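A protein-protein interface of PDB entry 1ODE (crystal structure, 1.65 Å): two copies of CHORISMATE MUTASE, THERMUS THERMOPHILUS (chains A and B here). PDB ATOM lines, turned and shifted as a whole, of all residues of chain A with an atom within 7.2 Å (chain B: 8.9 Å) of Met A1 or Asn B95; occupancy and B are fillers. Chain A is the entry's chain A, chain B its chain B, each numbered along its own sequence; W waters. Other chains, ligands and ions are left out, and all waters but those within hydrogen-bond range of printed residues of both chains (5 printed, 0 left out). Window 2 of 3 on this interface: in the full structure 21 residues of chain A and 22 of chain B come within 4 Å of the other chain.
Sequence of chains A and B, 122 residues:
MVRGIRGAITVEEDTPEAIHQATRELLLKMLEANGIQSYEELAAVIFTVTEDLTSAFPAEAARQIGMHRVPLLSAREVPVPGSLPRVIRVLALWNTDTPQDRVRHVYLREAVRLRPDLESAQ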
ATOM      1  N   MET A   1      22.595   2.403 -18.190  1.00  0.00           N
ATOM      2  CA  MET A   1      21.381   3.268 -18.175  1.00  0.00           C
ATOM      3  C   MET A   1      21.736   4.747 -18.304  1.00  0.00           C
ATOM      4  O   MET A   1      22.599   5.254 -17.593  1.00  0.00           O
ATOM      5  CB  MET A   1      20.595   3.048 -16.879  1.00  0.00           C
ATOM      6  CG  MET A   1      20.007   1.654 -16.722  1.00  0.00           C
ATOM      7  SD  MET A   1      18.826   1.253 -18.023  1.00  0.00           S
ATOM      8  CE  MET A   1      19.828   0.212 -19.087  1.00  0.00           C
ATOM      9  N   VAL A   2      21.067   5.436 -19.219  1.00  0.00           N
ATOM     10  CA  VAL A   2      21.313   6.859 -19.417  1.00  0.00           C
ATOM     11  C   VAL A   2      20.031   7.629 -19.156  1.00  0.00           C
ATOM     12  O   VAL A   2      18.967   7.256 -19.648  1.00  0.00           O
ATOM     13  CB  VAL A   2      21.778   7.159 -20.856  1.00  0.00           C
ATOM     14  CG1 VAL A   2      21.836   8.668 -21.091  1.00  0.00           C
ATOM     15  CG2 VAL A   2      23.140   6.533 -21.093  1.00  0.00           C
ATOM     16  N   ARG A   3      20.129   8.690 -18.368  1.00  0.00           N
ATOM     17  CA  ARG A   3      18.955   9.513 -18.092  1.00  0.00           C
ATOM     18  C   ARG A   3      19.283  10.938 -18.489  1.00  0.00           C
ATOM     19  O   ARG A   3      20.356  11.448 -18.167  1.00  0.00           O
ATOM     20  CB  ARG A   3      18.586   9.501 -16.604  1.00  0.00           C
ATOM     21  CG  ARG A   3      18.436   8.125 -15.973  1.00  0.00           C
ATOM     22  CD  ARG A   3      17.346   7.277 -16.603  1.00  0.00           C
ATOM     23  NE  ARG A   3      17.210   6.023 -15.866  1.00  0.00           N
ATOM     24  CZ  ARG A   3      16.657   4.914 -16.345  1.00  0.00           C
ATOM     25  NH1 ARG A   3      16.177   4.882 -17.579  1.00  0.00           N
ATOM     26  NH2 ARG A   3      16.592   3.828 -15.584  1.00  0.00           N
ATOM     27  N   GLY A   4      18.363  11.579 -19.196  1.00  0.00           N
ATOM     28  CA  GLY A   4      18.603  12.955 -19.573  1.00  0.00           C
ATOM     29  C   GLY A   4      18.205  13.859 -18.425  1.00  0.00           C
ATOM     30  O   GLY A   4      17.311  13.525 -17.648  1.00  0.00           O
ATOM     31  N   GLU A  41      30.490  10.909 -14.921  1.00  0.00           N
ATOM     32  CA  GLU A  41      29.185  10.270 -15.094  1.00  0.00           C
ATOM     33  C   GLU A  41      28.400  10.861 -16.271  1.00  0.00           C
ATOM     34  O   GLU A  41      27.387  10.296 -16.698  1.00  0.00           O
ATOM     35  CB  GLU A  41      28.343  10.461 -13.823  1.00  0.00           C
ATOM     36  CG  GLU A  41      28.996  10.017 -12.519  1.00  0.00           C
ATOM     37  CD  GLU A  41      28.211  10.466 -11.294  1.00  0.00           C
ATOM     38  OE1 GLU A  41      26.993  10.185 -11.219  1.00  0.00           O
ATOM     39  OE2 GLU A  41      28.812  11.104 -10.402  1.00  0.00           O
ATOM     40  N   TRP A  94      23.105  11.597 -18.581  1.00  0.00           N
ATOM     41  CA  TRP A  94      23.730  11.065 -17.374  1.00  0.00           C
ATOM     42  C   TRP A  94      23.732   9.546 -17.252  1.00  0.00           C
ATOM     43  O   TRP A  94      22.683   8.914 -17.339  1.00  0.00           O
ATOM     44  CB  TRP A  94      22.992  11.720 -16.198  1.00  0.00           C
ATOM     45  CG  TRP A  94      23.429  11.369 -14.821  1.00  0.00           C
ATOM     46  CD1 TRP A  94      24.690  11.069 -14.398  1.00  0.00           C
ATOM     47  CD2 TRP A  94      22.601  11.384 -13.652  1.00  0.00           C
ATOM     48  NE1 TRP A  94      24.699  10.899 -13.027  1.00  0.00           N
ATOM     49  CE2 TRP A  94      23.429  11.088 -12.548  1.00  0.00           C
ATOM     50  CE3 TRP A  94      21.236  11.624 -13.432  1.00  0.00           C
ATOM     51  CZ2 TRP A  94      22.935  11.026 -11.238  1.00  0.00           C
ATOM     52  CZ3 TRP A  94      20.743  11.563 -12.131  1.00  0.00           C
ATOM     53  CH2 TRP A  94      21.596  11.265 -11.048  1.00  0.00           C
ATOM     54  N   ASN A  95      24.921   8.963 -17.088  1.00  0.00           N
ATOM     55  CA  ASN A  95      25.034   7.515 -16.905  1.00  0.00           C
ATOM     56  C   ASN A  95      24.695   7.277 -15.432  1.00  0.00           C
ATOM     57  O   ASN A  95      25.444   7.679 -14.541  1.00  0.00           O
ATOM     58  CB  ASN A  95      26.460   7.041 -17.193  1.00  0.00           C
ATOM     59  CG  ASN A  95      26.794   7.049 -18.670  1.00  0.00           C
ATOM     60  OD1 ASN A  95      26.193   6.321 -19.455  1.00  0.00           O
ATOM     61  ND2 ASN A  95      27.762   7.870 -19.053  1.00  0.00           N
ATOM     62  N   THR A  96      23.561   6.637 -15.181  1.00  0.00           N
ATOM     63  CA  THR A  96      23.116   6.406 -13.814  1.00  0.00           C
ATOM     64  C   THR A  96      22.042   5.325 -13.780  1.00  0.00           C
ATOM     65  O   THR A  96      21.456   4.998 -14.809  1.00  0.00           O
ATOM     66  CB  THR A  96      22.514   7.713 -13.237  1.00  0.00           C
ATOM     67  OG1 THR A  96      22.139   7.518 -11.871  1.00  0.00           O
ATOM     68  CG2 THR A  96      21.282   8.123 -14.044  1.00  0.00           C
ATOM     69  N   ASP A  97      21.796   4.771 -12.596  1.00  0.00           N
ATOM     70  CA  ASP A  97      20.757   3.760 -12.430  1.00  0.00           C
ATOM     71  C   ASP A  97      19.505   4.456 -11.902  1.00  0.00           C
ATOM     72  O   ASP A  97      18.444   3.846 -11.778  1.00  0.00           O
ATOM     73  CB  ASP A  97      21.209   2.670 -11.453  1.00  0.00           C
ATOM     74  CG  ASP A  97      22.112   1.636 -12.104  1.00  0.00           C
ATOM     75  OD1 ASP A  97      22.610   0.745 -11.385  1.00  0.00           O
ATOM     76  OD2 ASP A  97      22.318   1.710 -13.335  1.00  0.00           O
ATOM     77  N   THR A  98      19.649   5.743 -11.598  1.00  0.00           N
ATOM     78  CA  THR A  98      18.546   6.558 -11.097  1.00  0.00           C
ATOM     79  C   THR A  98      17.345   6.428 -12.018  1.00  0.00           C
ATOM     80  O   THR A  98      17.459   6.624 -13.227  1.00  0.00           O
ATOM     81  CB  THR A  98      18.930   8.060 -11.042  1.00  0.00           C
ATOM     82  OG1 THR A  98      20.048   8.246 -10.167  1.00  0.00           O
ATOM     83  CG2 THR A  98      17.752   8.895 -10.550  1.00  0.00           C
ATOM     84  N   GLN A 100      13.877   7.257 -13.999  1.00  0.00           N
ATOM     85  CA  GLN A 100      13.421   8.461 -14.691  1.00  0.00           C
ATOM     86  C   GLN A 100      12.617   9.402 -13.798  1.00  0.00           C
ATOM     87  O   GLN A 100      12.783  10.618 -13.864  1.00  0.00           O
ATOM     88  CB  GLN A 100      12.566   8.063 -15.896  1.00  0.00           C
ATOM     89  CG  GLN A 100      12.203   9.202 -16.842  1.00  0.00           C
ATOM     90  CD  GLN A 100      11.271   8.744 -17.952  1.00  0.00           C
ATOM     91  OE1 GLN A 100      10.090   8.485 -17.715  1.00  0.00           O
ATOM     92  NE2 GLN A 100      11.802   8.623 -19.165  1.00  0.00           N
ATOM     93  N   MET B   1      22.435  -0.823 -22.831  1.00  0.00           N
ATOM     94  CA  MET B   1      22.962   0.070 -23.900  1.00  0.00           C
ATOM     95  C   MET B   1      21.928   1.105 -24.324  1.00  0.00           C
ATOM     96  O   MET B   1      20.767   1.037 -23.929  1.00  0.00           O
ATOM     97  CB  MET B   1      23.368  -0.749 -25.130  1.00  0.00           C
ATOM     98  CG  MET B   1      24.676  -1.512 -24.983  1.00  0.00           C
ATOM     99  SD  MET B   1      24.658  -2.667 -23.612  1.00  0.00           S
ATOM    100  CE  MET B   1      25.523  -1.709 -22.346  1.00  0.00           C
ATOM    101  N   VAL B   2      22.364   2.063 -25.134  1.00  0.00           N
ATOM    102  CA  VAL B   2      21.474   3.095 -25.641  1.00  0.00           C
ATOM    103  C   VAL B   2      21.445   2.988 -27.154  1.00  0.00           C
ATOM    104  O   VAL B   2      22.490   2.851 -27.803  1.00  0.00           O
ATOM    105  CB  VAL B   2      21.950   4.516 -25.245  1.00  0.00           C
ATOM    106  CG1 VAL B   2      21.105   5.568 -25.965  1.00  0.00           C
ATOM    107  CG2 VAL B   2      21.835   4.705 -23.741  1.00  0.00           C
ATOM    108  N   ARG B   3      20.244   3.023 -27.717  1.00  0.00           N
ATOM    109  CA  ARG B   3      20.091   2.955 -29.162  1.00  0.00           C
ATOM    110  C   ARG B   3      19.216   4.119 -29.555  1.00  0.00           C
ATOM    111  O   ARG B   3      18.199   4.373 -28.916  1.00  0.00           O
ATOM    112  CB  ARG B   3      19.375   1.672 -29.592  1.00  0.00           C
ATOM    113  CG  ARG B   3      19.955   0.388 -29.028  1.00  0.00           C
ATOM    114  CD  ARG B   3      21.363   0.096 -29.515  1.00  0.00           C
ATOM    115  NE  ARG B   3      21.777  -1.236 -29.078  1.00  0.00           N
ATOM    116  CZ  ARG B   3      23.037  -1.616 -28.889  1.00  0.00           C
ATOM    117  NH1 ARG B   3      24.031  -0.766 -29.099  1.00  0.00           N
ATOM    118  NH2 ARG B   3      23.302  -2.850 -28.480  1.00  0.00           N
ATOM    119  N   GLY B   4      19.605   4.829 -30.602  1.00  0.00           N
ATOM    120  CA  GLY B   4      18.784   5.935 -31.042  1.00  0.00           C
ATOM    121  C   GLY B   4      17.706   5.402 -31.966  1.00  0.00           C
ATOM    122  O   GLY B   4      17.910   4.401 -32.660  1.00  0.00           O
ATOM    123  N   ILE B   5      16.544   6.046 -31.938  1.00  0.00           N
ATOM    124  CA  ILE B   5      15.430   5.679 -32.806  1.00  0.00           C
ATOM    125  C   ILE B   5      15.132   6.931 -33.614  1.00  0.00           C
ATOM    126  O   ILE B   5      14.931   8.010 -33.045  1.00  0.00           O
ATOM    127  CB  ILE B   5      14.151   5.315 -32.022  1.00  0.00           C
ATOM    128  CG1 ILE B   5      14.446   4.249 -30.966  1.00  0.00           C
ATOM    129  CG2 ILE B   5      13.088   4.785 -32.999  1.00  0.00           C
ATOM    130  CD1 ILE B   5      13.247   3.920 -30.083  1.00  0.00           C
ATOM    131  N   ILE B  36       7.589  -0.491 -27.409  1.00  0.00           N
ATOM    132  CA  ILE B  36       7.797   0.264 -26.184  1.00  0.00           C
ATOM    133  C   ILE B  36       6.438   0.659 -25.604  1.00  0.00           C
ATOM    134  O   ILE B  36       5.731   1.486 -26.176  1.00  0.00           O
ATOM    135  CB  ILE B  36       8.637   1.530 -26.460  1.00  0.00           C
ATOM    136  CG1 ILE B  36       9.961   1.133 -27.120  1.00  0.00           C
ATOM    137  CG2 ILE B  36       8.906   2.273 -25.164  1.00  0.00           C
ATOM    138  CD1 ILE B  36      10.750   2.303 -27.662  1.00  0.00           C
ATOM    139  N   SER B  38       6.126   1.706 -22.312  1.00  0.00           N
ATOM    140  CA  SER B  38       6.356   2.637 -21.212  1.00  0.00           C
ATOM    141  C   SER B  38       7.395   3.685 -21.600  1.00  0.00           C
ATOM    142  O   SER B  38       8.302   3.413 -22.387  1.00  0.00           O
ATOM    143  CB  SER B  38       6.830   1.880 -19.970  1.00  0.00           C
ATOM    144  OG  SER B  38       7.161   2.773 -18.917  1.00  0.00           O
ATOM    145  N   TYR B  39       7.263   4.881 -21.042  1.00  0.00           N
ATOM    146  CA  TYR B  39       8.199   5.961 -21.347  1.00  0.00           C
ATOM    147  C   TYR B  39       9.453   5.916 -20.479  1.00  0.00           C
ATOM    148  O   TYR B  39      10.408   6.652 -20.729  1.00  0.00           O
ATOM    149  CB  TYR B  39       7.519   7.324 -21.171  1.00  0.00           C
ATOM    150  CG  TYR B  39       6.293   7.545 -22.031  1.00  0.00           C
ATOM    151  CD1 TYR B  39       6.289   7.192 -23.380  1.00  0.00           C
ATOM    152  CD2 TYR B  39       5.151   8.155 -21.507  1.00  0.00           C
ATOM    153  CE1 TYR B  39       5.178   7.443 -24.191  1.00  0.00           C
ATOM    154  CE2 TYR B  39       4.032   8.413 -22.310  1.00  0.00           C
ATOM    155  CZ  TYR B  39       4.057   8.055 -23.652  1.00  0.00           C
ATOM    156  OH  TYR B  39       2.976   8.328 -24.462  1.00  0.00           O
ATOM    157  N   GLU B  40       9.455   5.054 -19.465  1.00  0.00           N
ATOM    158  CA  GLU B  40      10.596   4.937 -18.564  1.00  0.00           C
ATOM    159  C   GLU B  40      11.883   4.519 -19.264  1.00  0.00           C
ATOM    160  O   GLU B  40      12.971   4.746 -18.743  1.00  0.00           O
ATOM    161  CB  GLU B  40      10.295   3.935 -17.443  1.00  0.00           C
ATOM    162  CG  GLU B  40       9.357   4.456 -16.365  1.00  0.00           C
ATOM    163  CD  GLU B  40       9.112   3.432 -15.269  1.00  0.00           C
ATOM    164  OE1 GLU B  40       8.522   2.372 -15.565  1.00  0.00           O
ATOM    165  OE2 GLU B  40       9.514   3.686 -14.112  1.00  0.00           O
ATOM    166  N   GLU B  41      11.752   3.919 -20.442  1.00  0.00           N
ATOM    167  CA  GLU B  41      12.900   3.449 -21.218  1.00  0.00           C
ATOM    168  C   GLU B  41      13.582   4.553 -22.027  1.00  0.00           C
ATOM    169  O   GLU B  41      14.711   4.390 -22.491  1.00  0.00           O
ATOM    170  CB  GLU B  41      12.456   2.333 -22.171  1.00  0.00           C
ATOM    171  CG  GLU B  41      11.940   1.072 -21.480  1.00  0.00           C
ATOM    172  CD  GLU B  41      11.221   0.132 -22.437  1.00  0.00           C
ATOM    173  OE1 GLU B  41      11.827  -0.280 -23.448  1.00  0.00           O
ATOM    174  OE2 GLU B  41      10.043  -0.194 -22.176  1.00  0.00           O
ATOM    175  N   LEU B  42      12.904   5.682 -22.193  1.00  0.00           N
ATOM    176  CA  LEU B  42      13.465   6.772 -22.979  1.00  0.00           C
ATOM    177  C   LEU B  42      14.380   7.691 -22.187  1.00  0.00           C
ATOM    178  O   LEU B  42      13.936   8.385 -21.273  1.00  0.00           O
ATOM    179  CB  LEU B  42      12.332   7.581 -23.611  1.00  0.00           C
ATOM    180  CG  LEU B  42      11.378   6.763 -24.482  1.00  0.00           C
ATOM    181  CD1 LEU B  42      10.262   7.665 -24.990  1.00  0.00           C
ATOM    182  CD2 LEU B  42      12.155   6.130 -25.642  1.00  0.00           C
ATOM    183  N   ALA B  43      15.661   7.694 -22.548  1.00  0.00           N
ATOM    184  CA  ALA B  43      16.636   8.549 -21.886  1.00  0.00           C
ATOM    185  C   ALA B  43      16.301  10.005 -22.180  1.00  0.00           C
ATOM    186  O   ALA B  43      16.398  10.865 -21.308  1.00  0.00           O
ATOM    187  CB  ALA B  43      18.043   8.234 -22.393  1.00  0.00           C
ATOM    188  N   ALA B  44      15.909  10.270 -23.424  1.00  0.00           N
ATOM    189  CA  ALA B  44      15.563  11.618 -23.851  1.00  0.00           C
ATOM    190  C   ALA B  44      15.076  11.582 -25.287  1.00  0.00           C
ATOM    191  O   ALA B  44      15.280  10.599 -25.997  1.00  0.00           O
ATOM    192  CB  ALA B  44      16.785  12.531 -23.751  1.00  0.00           C
ATOM    193  N   PRO B  71      12.893  13.636 -20.786  1.00  0.00           N
ATOM    194  CA  PRO B  71      13.618  14.871 -21.118  1.00  0.00           C
ATOM    195  C   PRO B  71      13.492  15.153 -22.617  1.00  0.00           C
ATOM    196  O   PRO B  71      13.764  14.279 -23.446  1.00  0.00           O
ATOM    197  CB  PRO B  71      15.057  14.549 -20.719  1.00  0.00           C
ATOM    198  CG  PRO B  71      14.891  13.563 -19.614  1.00  0.00           C
ATOM    199  CD  PRO B  71      13.782  12.671 -20.121  1.00  0.00           C
ATOM    200  N   ALA B  92      15.011   9.642 -30.635  1.00  0.00           N
ATOM    201  CA  ALA B  92      14.758   9.202 -29.275  1.00  0.00           C
ATOM    202  C   ALA B  92      15.953   8.350 -28.858  1.00  0.00           C
ATOM    203  O   ALA B  92      16.433   7.532 -29.637  1.00  0.00           O
ATOM    204  CB  ALA B  92      13.474   8.377 -29.217  1.00  0.00           C
ATOM    205  N   LEU B  93      16.458   8.577 -27.652  1.00  0.00           N
ATOM    206  CA  LEU B  93      17.573   7.790 -27.143  1.00  0.00           C
ATOM    207  C   LEU B  93      16.899   6.764 -26.239  1.00  0.00           C
ATOM    208  O   LEU B  93      16.319   7.109 -25.212  1.00  0.00           O
ATOM    209  CB  LEU B  93      18.551   8.692 -26.384  1.00  0.00           C
ATOM    210  CG  LEU B  93      19.225   9.711 -27.321  1.00  0.00           C
ATOM    211  CD1 LEU B  93      20.127  10.660 -26.535  1.00  0.00           C
ATOM    212  CD2 LEU B  93      20.033   8.970 -28.377  1.00  0.00           C
ATOM    213  N   TRP B  94      16.975   5.499 -26.647  1.00  0.00           N
ATOM    214  CA  TRP B  94      16.310   4.404 -25.951  1.00  0.00           C
ATOM    215  C   TRP B  94      17.231   3.464 -25.173  1.00  0.00           C
ATOM    216  O   TRP B  94      18.202   2.937 -25.724  1.00  0.00           O
ATOM    217  CB  TRP B  94      15.502   3.630 -27.004  1.00  0.00           C
ATOM    218  CG  TRP B  94      14.730   2.419 -26.545  1.00  0.00           C
ATOM    219  CD1 TRP B  94      14.165   2.206 -25.321  1.00  0.00           C
ATOM    220  CD2 TRP B  94      14.382   1.283 -27.351  1.00  0.00           C
ATOM    221  NE1 TRP B  94      13.483   1.005 -25.314  1.00  0.00           N
ATOM    222  CE2 TRP B  94      13.602   0.421 -26.548  1.00  0.00           C
ATOM    223  CE3 TRP B  94      14.652   0.914 -28.675  1.00  0.00           C
ATOM    224  CZ2 TRP B  94      13.090  -0.792 -27.028  1.00  0.00           C
ATOM    225  CZ3 TRP B  94      14.144  -0.292 -29.152  1.00  0.00           C
ATOM    226  CH2 TRP B  94      13.371  -1.130 -28.328  1.00  0.00           C
ATOM    227  N   ASN B  95      16.933   3.277 -23.888  1.00  0.00           N
ATOM    228  CA  ASN B  95      17.714   2.364 -23.048  1.00  0.00           C
ATOM    229  C   ASN B  95      17.165   0.984 -23.375  1.00  0.00           C
ATOM    230  O   ASN B  95      16.030   0.664 -23.016  1.00  0.00           O
ATOM    231  CB  ASN B  95      17.493   2.651 -21.562  1.00  0.00           C
ATOM    232  CG  ASN B  95      18.193   3.907 -21.102  1.00  0.00           C
ATOM    233  OD1 ASN B  95      19.412   4.041 -21.242  1.00  0.00           O
ATOM    234  ND2 ASN B  95      17.431   4.833 -20.538  1.00  0.00           N
ATOM    235  N   THR B  96      17.963   0.171 -24.053  1.00  0.00           N
ATOM    236  CA  THR B  96      17.503  -1.157 -24.446  1.00  0.00           C
ATOM    237  C   THR B  96      18.644  -2.123 -24.734  1.00  0.00           C
ATOM    238  O   THR B  96      19.786  -1.716 -24.947  1.00  0.00           O
ATOM    239  CB  THR B  96      16.614  -1.058 -25.712  1.00  0.00           C
ATOM    240  OG1 THR B  96      16.131  -2.357 -26.072  1.00  0.00           O
ATOM    241  CG2 THR B  96      17.413  -0.494 -26.879  1.00  0.00           C
ATOM    242  N   ASP B  97      18.315  -3.410 -24.739  1.00  0.00           N
ATOM    243  CA  ASP B  97      19.283  -4.461 -25.023  1.00  0.00           C
ATOM    244  C   ASP B  97      19.180  -4.785 -26.510  1.00  0.00           C
ATOM    245  O   ASP B  97      19.999  -5.521 -27.060  1.00  0.00           O
ATOM    246  CB  ASP B  97      18.959  -5.706 -24.193  1.00  0.00           C
ATOM    247  CG  ASP B  97      17.555  -6.231 -24.450  1.00  0.00           C
ATOM    248  OD1 ASP B  97      17.285  -6.702 -25.576  1.00  0.00           O
ATOM    249  OD2 ASP B  97      16.716  -6.168 -23.526  1.00  0.00           O
ATOM    250  N   THR B  98      18.158  -4.224 -27.148  1.00  0.00           N
ATOM    251  CA  THR B  98      17.909  -4.431 -28.569  1.00  0.00           C
ATOM    252  C   THR B  98      19.119  -4.044 -29.411  1.00  0.00           C
ATOM    253  O   THR B  98      19.663  -2.950 -29.265  1.00  0.00           O
ATOM    254  CB  THR B  98      16.710  -3.580 -29.055  1.00  0.00           C
ATOM    255  OG1 THR B  98      15.555  -3.870 -28.261  1.00  0.00           O
ATOM    256  CG2 THR B  98      16.402  -3.879 -30.515  1.00  0.00           C
HETATM  257  O   HOH W   1      15.004   6.666 -18.981  1.00  0.00           O
HETATM  258  O   HOH W   2      21.129   1.760 -21.277  1.00  0.00           O
HETATM  259  O   HOH W   3      13.204   5.001 -15.641  1.00  0.00           O
HETATM  260  O   HOH W   4      14.819   9.348 -18.873  1.00  0.00           O
HETATM  261  O   HOH W   5      15.436   2.582 -18.697  1.00  0.00           O
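The backbone NH (N) of Val A2 lies within hydrogen-bond range of the side-chain amide oxygen (OD1) of Asn B95, 3.0 Å away.
O of Ala B43 sits at hydrogen-bond distance from N of Gly A4 (3.0 Å).
ND2 of Asn B95 sits close to NH1 of Arg A3.
The side-chain amide nitrogen of Gln A100 sits at hydrogen-bond distance from the backbone carbonyl oxygen of Leu B42 (3.0 Å).
The guanidinium group (NH1) of Arg A3 is in hydrogen-bond range of the backbone carbonyl oxygen (O) of Glu B40.
The backbone carbonyl oxygen (O) of Tyr B39 lies within hydrogen-bond range of the side-chain amide nitrogen (NE2) of Gln A100 (2.9 Å).
Of the 11 printed residues of chain A, 5 touch a printed residue of chain B.
Hydrophobic or aromatic side chains of chain A that line the printed part of chain B: Val A2.
Met A1 touches just one residue of chain B: Asn B95 (3.7 Å).
Printed residues of chain B within 4 Å of Val A2: Val B2 (3.5 Å), Ala B43 (3.1 Å) and Asn B95 (3.0 Å).
Printed residues of chain B within 4 Å of Gly A4: Ala B43 (3.0 Å) and Pro B71 (3.1 Å).
Printed residues of chain B within 4 Å of Gln A100: Tyr B39, Glu B40 and Leu B42.
Printed residues of chain A within 4 Å of Ala B43: Val A2 and Gly A4.
Of chain A, only Met A1 (3.7 Å), Val A2 (3.0 Å) and Arg A3 (3.2 Å) come within 4 Å of Asn B95.
The nearest residue of chain A that does not touch Asn B95 is Thr A96 (6.8 Å).
The nearest printed residue of chain A that does not touch Pro B71 is Gln A100 (4.6 Å).
Water W1 lies within hydrogen-bond range of the guanidinium group of Arg A3 (2.6 Å), the backbone carbonyl oxygen of Glu B40 (2.8 Å), the backbone carbonyl oxygen of Leu B42 (3.1 Å) and the side-chain amide nitrogen of Asn B95 (3.4 Å).
Water W5 lies within hydrogen-bond range of the guanidinium group of Arg A3 (2.7 Å), the backbone carbonyl oxygen of Glu B40 (3.3 Å) and the side-chain sulfur of Met A1 (3.7 Å).
Water W4 lies within hydrogen-bond range of the backbone carbonyl oxygen (O) of Leu B42 (2.7 Å), the side-chain amide nitrogen (NE2) of Gln A100 (3.1 Å) and the backbone carbonyl oxygen (O) of Ala B43 (3.3 Å).
Water W2 lies within hydrogen-bond range of O of Met B1, OD1 of Asn B95 and N of Met A1.
Water W3 lies within hydrogen-bond range of N of Gln A100 (2.9 Å) and O of Glu B40 (3.1 Å).
Among the printed residues, pairs that only touch across the chains: Met A1 with Asn B95 (3.7 Å), Val A2 with Val B2 (3.5 Å), Val A2 with Ala B43 (3.1 Å), Gly A4 with Pro B71 (3.1 Å) and Gln A100 with Glu B40 (3.7 Å).
Met A1 touches Asn B95, but with the chains exchanged Asn A95 does not touch Met B1 (8.3 Å).
Val A2 touches its own counterpart, Val B2.
Val A2 touches Asn B95, but with the chains exchanged Asn A95 does not touch Val B2 (6.3 Å).
Arg A3 touches Asn B95, but with the chains exchanged Asn A95 does not touch Arg B3 (10.7 Å).
The backbone NH (N) of Ala B43 sits at hydrogen-bond distance from the backbone carbonyl oxygen (O) of Leu B93, at 2.8 Å.
O of Glu B41 lies within hydrogen-bond range of N of Asn B95 (2.9 Å).
The backbone NH (N) of Thr A96 lies within hydrogen-bond range of the backbone carbonyl oxygen (O) of Met A1 (2.9 Å).
N of Arg A3 lies within hydrogen-bond range of O of Trp A94 (2.8 Å).
N of Glu B40 sits close to OG of Ser B38 (3.3 Å).
The guanidinium group of Arg A3 is in hydrogen-bond range of the backbone carbonyl oxygen of Thr A98, 2.7 Å away.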
